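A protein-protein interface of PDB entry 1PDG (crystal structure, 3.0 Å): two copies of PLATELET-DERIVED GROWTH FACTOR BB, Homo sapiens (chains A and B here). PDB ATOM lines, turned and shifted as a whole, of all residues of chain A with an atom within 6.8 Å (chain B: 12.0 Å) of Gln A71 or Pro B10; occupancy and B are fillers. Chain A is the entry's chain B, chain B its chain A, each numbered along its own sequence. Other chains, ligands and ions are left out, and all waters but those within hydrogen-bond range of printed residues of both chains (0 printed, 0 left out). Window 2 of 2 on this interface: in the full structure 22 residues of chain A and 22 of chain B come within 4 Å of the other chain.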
ATOM      1  N   TRP A  40      16.301  12.495   1.924  1.00  0.00           N
ATOM      2  CA  TRP A  40      15.952  13.542   2.854  1.00  0.00           C
ATOM      3  C   TRP A  40      15.354  12.853   4.109  1.00  0.00           C
ATOM      4  O   TRP A  40      14.276  12.272   3.969  1.00  0.00           O
ATOM      5  CB  TRP A  40      15.025  14.686   2.434  1.00  0.00           C
ATOM      6  CG  TRP A  40      15.541  15.980   3.008  1.00  0.00           C
ATOM      7  CD1 TRP A  40      16.476  16.812   2.450  1.00  0.00           C
ATOM      8  CD2 TRP A  40      15.278  16.490   4.310  1.00  0.00           C
ATOM      9  NE1 TRP A  40      16.775  17.848   3.319  1.00  0.00           N
ATOM     10  CE2 TRP A  40      16.051  17.677   4.454  1.00  0.00           C
ATOM     11  CE3 TRP A  40      14.448  16.078   5.343  1.00  0.00           C
ATOM     12  CZ2 TRP A  40      16.025  18.451   5.603  1.00  0.00           C
ATOM     13  CZ3 TRP A  40      14.385  16.877   6.491  1.00  0.00           C
ATOM     14  CH2 TRP A  40      15.162  18.031   6.622  1.00  0.00           C
ATOM     15  N   PRO A  41      16.083  12.829   5.192  1.00  0.00           N
ATOM     16  CA  PRO A  41      17.410  13.372   5.425  1.00  0.00           C
ATOM     17  C   PRO A  41      18.609  12.670   4.786  1.00  0.00           C
ATOM     18  O   PRO A  41      18.797  11.468   5.023  1.00  0.00           O
ATOM     19  CB  PRO A  41      17.567  13.088   6.965  1.00  0.00           C
ATOM     20  CG  PRO A  41      16.835  11.752   7.066  1.00  0.00           C
ATOM     21  CD  PRO A  41      15.516  12.109   6.378  1.00  0.00           C
ATOM     22  N   PRO A  69      17.166   1.224  12.888  1.00  0.00           N
ATOM     23  CA  PRO A  69      16.632   1.435  11.515  1.00  0.00           C
ATOM     24  C   PRO A  69      15.967   2.808  11.589  1.00  0.00           C
ATOM     25  O   PRO A  69      15.436   3.085  12.689  1.00  0.00           O
ATOM     26  CB  PRO A  69      15.592   0.327  11.470  1.00  0.00           C
ATOM     27  CG  PRO A  69      14.984   0.385  12.864  1.00  0.00           C
ATOM     28  CD  PRO A  69      16.178   0.586  13.772  1.00  0.00           C
ATOM     29  N   VAL A  70      16.037   3.598  10.574  1.00  0.00           N
ATOM     30  CA  VAL A  70      15.446   4.955  10.549  1.00  0.00           C
ATOM     31  C   VAL A  70      14.579   5.031   9.291  1.00  0.00           C
ATOM     32  O   VAL A  70      15.031   4.437   8.283  1.00  0.00           O
ATOM     33  CB  VAL A  70      16.550   6.030  10.579  1.00  0.00           C
ATOM     34  CG1 VAL A  70      17.685   5.708  11.535  1.00  0.00           C
ATOM     35  CG2 VAL A  70      17.119   6.358   9.198  1.00  0.00           C
ATOM     36  N   GLN A  71      13.433   5.686   9.397  1.00  0.00           N
ATOM     37  CA  GLN A  71      12.583   5.819   8.180  1.00  0.00           C
ATOM     38  C   GLN A  71      13.066   7.076   7.438  1.00  0.00           C
ATOM     39  O   GLN A  71      13.437   8.069   8.071  1.00  0.00           O
ATOM     40  CB  GLN A  71      11.138   5.630   8.284  1.00  0.00           C
ATOM     41  CG  GLN A  71      10.406   5.760   9.590  1.00  0.00           C
ATOM     42  CD  GLN A  71       8.945   6.156   9.356  1.00  0.00           C
ATOM     43  OE1 GLN A  71       8.617   6.852   8.387  1.00  0.00           O
ATOM     44  NE2 GLN A  71       8.111   5.655  10.270  1.00  0.00           N
ATOM     45  N   VAL A  72      13.072   6.953   6.133  1.00  0.00           N
ATOM     46  CA  VAL A  72      13.666   7.945   5.223  1.00  0.00           C
ATOM     47  C   VAL A  72      12.741   8.381   4.127  1.00  0.00           C
ATOM     48  O   VAL A  72      12.186   7.428   3.513  1.00  0.00           O
ATOM     49  CB  VAL A  72      14.851   7.080   4.601  1.00  0.00           C
ATOM     50  CG1 VAL A  72      15.190   7.498   3.199  1.00  0.00           C
ATOM     51  CG2 VAL A  72      16.021   7.004   5.537  1.00  0.00           C
ATOM     52  N   ARG A  73      12.647   9.639   3.763  1.00  0.00           N
ATOM     53  CA  ARG A  73      11.754   9.982   2.603  1.00  0.00           C
ATOM     54  C   ARG A  73      12.473   9.579   1.317  1.00  0.00           C
ATOM     55  O   ARG A  73      13.572  10.047   0.984  1.00  0.00           O
ATOM     56  CB  ARG A  73      11.253  11.395   2.620  1.00  0.00           C
ATOM     57  CG  ARG A  73      10.005  11.632   3.473  1.00  0.00           C
ATOM     58  CD  ARG A  73       9.888  13.050   3.947  1.00  0.00           C
ATOM     59  NE  ARG A  73       9.628  13.082   5.392  1.00  0.00           N
ATOM     60  CZ  ARG A  73      10.430  12.508   6.297  1.00  0.00           C
ATOM     61  NH1 ARG A  73      11.549  11.868   5.967  1.00  0.00           N
ATOM     62  NH2 ARG A  73      10.101  12.535   7.596  1.00  0.00           N
ATOM     63  N   LYS A  86       8.729   5.934   0.896  1.00  0.00           N
ATOM     64  CA  LYS A  86       9.346   5.898   2.196  1.00  0.00           C
ATOM     65  C   LYS A  86      10.051   4.538   2.421  1.00  0.00           C
ATOM     66  O   LYS A  86       9.423   3.496   2.623  1.00  0.00           O
ATOM     67  CB  LYS A  86       8.502   6.139   3.403  1.00  0.00           C
ATOM     68  CG  LYS A  86       7.153   6.732   3.358  1.00  0.00           C
ATOM     69  CD  LYS A  86       6.257   6.326   4.519  1.00  0.00           C
ATOM     70  CE  LYS A  86       5.770   4.912   4.504  1.00  0.00           C
ATOM     71  NZ  LYS A  86       4.785   4.587   3.426  1.00  0.00           N
ATOM     72  N   ALA A  87      11.353   4.640   2.523  1.00  0.00           N
ATOM     73  CA  ALA A  87      12.298   3.574   2.812  1.00  0.00           C
ATOM     74  C   ALA A  87      12.632   3.515   4.309  1.00  0.00           C
ATOM     75  O   ALA A  87      12.169   4.325   5.128  1.00  0.00           O
ATOM     76  CB  ALA A  87      13.589   3.845   2.020  1.00  0.00           C
ATOM     77  N   THR A  88      13.428   2.505   4.621  1.00  0.00           N
ATOM     78  CA  THR A  88      13.945   2.261   5.983  1.00  0.00           C
ATOM     79  C   THR A  88      15.439   1.912   5.840  1.00  0.00           C
ATOM     80  O   THR A  88      15.786   1.023   5.036  1.00  0.00           O
ATOM     81  CB  THR A  88      13.164   1.215   6.835  1.00  0.00           C
ATOM     82  OG1 THR A  88      13.545  -0.125   6.367  1.00  0.00           O
ATOM     83  CG2 THR A  88      11.627   1.371   6.856  1.00  0.00           C
ATOM     84  N   VAL A  89      16.255   2.658   6.561  1.00  0.00           N
ATOM     85  CA  VAL A  89      17.732   2.469   6.452  1.00  0.00           C
ATOM     86  C   VAL A  89      18.310   2.297   7.835  1.00  0.00           C
ATOM     87  O   VAL A  89      18.239   3.231   8.654  1.00  0.00           O
ATOM     88  CB  VAL A  89      18.261   3.664   5.651  1.00  0.00           C
ATOM     89  CG1 VAL A  89      18.001   4.975   6.387  1.00  0.00           C
ATOM     90  CG2 VAL A  89      19.683   3.514   5.210  1.00  0.00           C
ATOM     91  N   GLU B   9       9.323   8.571  15.507  1.00  0.00           N
ATOM     92  CA  GLU B   9      10.206   9.520  14.766  1.00  0.00           C
ATOM     93  C   GLU B   9      11.305   8.822  13.969  1.00  0.00           C
ATOM     94  O   GLU B   9      12.180   8.008  14.433  1.00  0.00           O
ATOM     95  CB  GLU B   9      10.868  10.573  15.675  1.00  0.00           C
ATOM     96  CG  GLU B   9      12.215  10.228  16.308  1.00  0.00           C
ATOM     97  CD  GLU B   9      12.331   8.939  17.080  1.00  0.00           C
ATOM     98  OE1 GLU B   9      11.238   8.523  17.598  1.00  0.00           O
ATOM     99  OE2 GLU B   9      13.370   8.300  17.303  1.00  0.00           O
ATOM    100  N   PRO B  10      11.309   9.145  12.683  1.00  0.00           N
ATOM    101  CA  PRO B  10      12.280   8.633  11.708  1.00  0.00           C
ATOM    102  C   PRO B  10      13.566   9.443  11.848  1.00  0.00           C
ATOM    103  O   PRO B  10      13.833  10.091  12.877  1.00  0.00           O
ATOM    104  CB  PRO B  10      11.636   8.865  10.369  1.00  0.00           C
ATOM    105  CG  PRO B  10      10.198   9.280  10.658  1.00  0.00           C
ATOM    106  CD  PRO B  10      10.343  10.029  12.008  1.00  0.00           C
ATOM    107  N   ALA B  11      14.327   9.376  10.764  1.00  0.00           N
ATOM    108  CA  ALA B  11      15.663  10.018  10.717  1.00  0.00           C
ATOM    109  C   ALA B  11      15.530  11.500  10.434  1.00  0.00           C
ATOM    110  O   ALA B  11      14.789  11.907   9.529  1.00  0.00           O
ATOM    111  CB  ALA B  11      16.533   9.343   9.663  1.00  0.00           C
ATOM    112  N   MET B  12      16.301  12.241  11.176  1.00  0.00           N
ATOM    113  CA  MET B  12      16.356  13.703  11.026  1.00  0.00           C
ATOM    114  C   MET B  12      17.817  14.063  10.706  1.00  0.00           C
ATOM    115  O   MET B  12      18.735  13.339  11.100  1.00  0.00           O
ATOM    116  CB  MET B  12      15.754  14.473  12.176  1.00  0.00           C
ATOM    117  CG  MET B  12      15.775  13.746  13.476  1.00  0.00           C
ATOM    118  SD  MET B  12      16.345  14.875  14.784  1.00  0.00           S
ATOM    119  CE  MET B  12      17.318  13.724  15.819  1.00  0.00           C
ATOM    120  N   ILE B  13      17.966  15.123   9.986  1.00  0.00           N
ATOM    121  CA  ILE B  13      19.217  15.683   9.544  1.00  0.00           C
ATOM    122  C   ILE B  13      20.143  16.038  10.698  1.00  0.00           C
ATOM    123  O   ILE B  13      19.730  16.363  11.827  1.00  0.00           O
ATOM    124  CB  ILE B  13      18.766  16.966   8.755  1.00  0.00           C
ATOM    125  CG1 ILE B  13      19.725  17.234   7.581  1.00  0.00           C
ATOM    126  CG2 ILE B  13      18.599  18.199   9.681  1.00  0.00           C
ATOM    127  CD1 ILE B  13      19.169  18.430   6.696  1.00  0.00           C
ATOM    128  N   ALA B  14      21.442  16.063  10.400  1.00  0.00           N
ATOM    129  CA  ALA B  14      22.527  16.432  11.283  1.00  0.00           C
ATOM    130  C   ALA B  14      22.838  17.926  11.101  1.00  0.00           C
ATOM    131  O   ALA B  14      23.608  18.241  10.210  1.00  0.00           O
ATOM    132  CB  ALA B  14      23.816  15.671  10.976  1.00  0.00           C
ATOM    133  N   GLU B  15      22.185  18.730  11.896  1.00  0.00           N
ATOM    134  CA  GLU B  15      22.365  20.203  11.897  1.00  0.00           C
ATOM    135  C   GLU B  15      23.773  20.469  11.406  1.00  0.00           C
ATOM    136  O   GLU B  15      24.621  19.584  11.771  1.00  0.00           O
ATOM    137  CB  GLU B  15      22.206  20.694  13.323  1.00  0.00           C
ATOM    138  CG  GLU B  15      22.821  19.948  14.466  1.00  0.00           C
ATOM    139  CD  GLU B  15      22.269  18.631  14.853  1.00  0.00           C
ATOM    140  OE1 GLU B  15      21.348  18.158  14.117  1.00  0.00           O
ATOM    141  OE2 GLU B  15      22.584  17.950  15.839  1.00  0.00           O
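Of the printed residues of chain B, Trp A40 touches Ile B13.
Pro A41 touches three residues of chain B.
Of chain B, only Ala B11 comes within 4 Å of Val A70.
Gln A71 touches two residues of chain B.
No residue of chain B comes within 4 Å of Val A72.
No residue of chain B comes within 4 Å of Arg A73.
No residue of chain B comes within 4 Å of Lys A86.
No residue of chain B comes within 4 Å of Ala A87.
No residue of chain B comes within 4 Å of Thr A88.
Pro B10 touches just one residue of chain A: Gln A71 (3.0 Å).
Of the printed residues of chain A, Met B12 touches Pro A41.
Printed residues of chain A within 4 Å of Ile B13: Trp A40 and Pro A41.
Ala B14 touches none of the printed residues of chain A.
The nearest residue of chain B that does not touch Gln A71 is Glu B9 (5.4 Å).
No position is printed for both chains.
Of the 7 pairs that touch across the chains among the printed residues, none has its exchanged pair printed and touching as well.
Ile B13 touches Trp A40 (CD1 to CZ2, 3.3 Å).
Ala B11 touches Pro A41 (O to CG, 3.2 Å).
Met B12 touches Pro A41 (C to CB, 3.9 Å).
Ile B13 touches Pro A41 (N to CB, 3.7 Å).
Ala B11 touches Val A70.
Pro B10 touches Gln A71.
The backbone NH (N) of Ala B11 lies within hydrogen-bond range of the backbone carbonyl oxygen (O) of Gln A71 (3.1 Å).
Of the 7 printed residues of chain B, 4 touch a printed residue of chain A.
Printed residues of chain B that touch a printed residue of chain A: Pro B10, Ala B11, Met B12 and Ile B13.
Hydrophobic or aromatic side chains of chain B within 4 Å of the printed part of chain A: Pro B10, Ala B11 and Ile B13.
Along chain B the printed residues that touch a printed residue of chain A span positions 10 to 13.
Of the 11 printed residues of chain A, 4 touch a printed residue of chain B.
Hydrophobic or aromatic side chains of chain A within 4 Å of the printed part of chain B: Trp A40, Pro A41 and Val A70.
Among the printed residues, 7 pairs touch across the chains.
Among the printed residues, no Asp or Glu carboxylate lies within 4 Å of a Lys or Arg side-chain nitrogen of the other chain.
N of Val A89 is in hydrogen-bond range of O of Val A70.
The backbone NH (N) of Arg A73 sits at hydrogen-bond distance from the backbone carbonyl oxygen (O) of Trp A40, at 3.1 Å.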
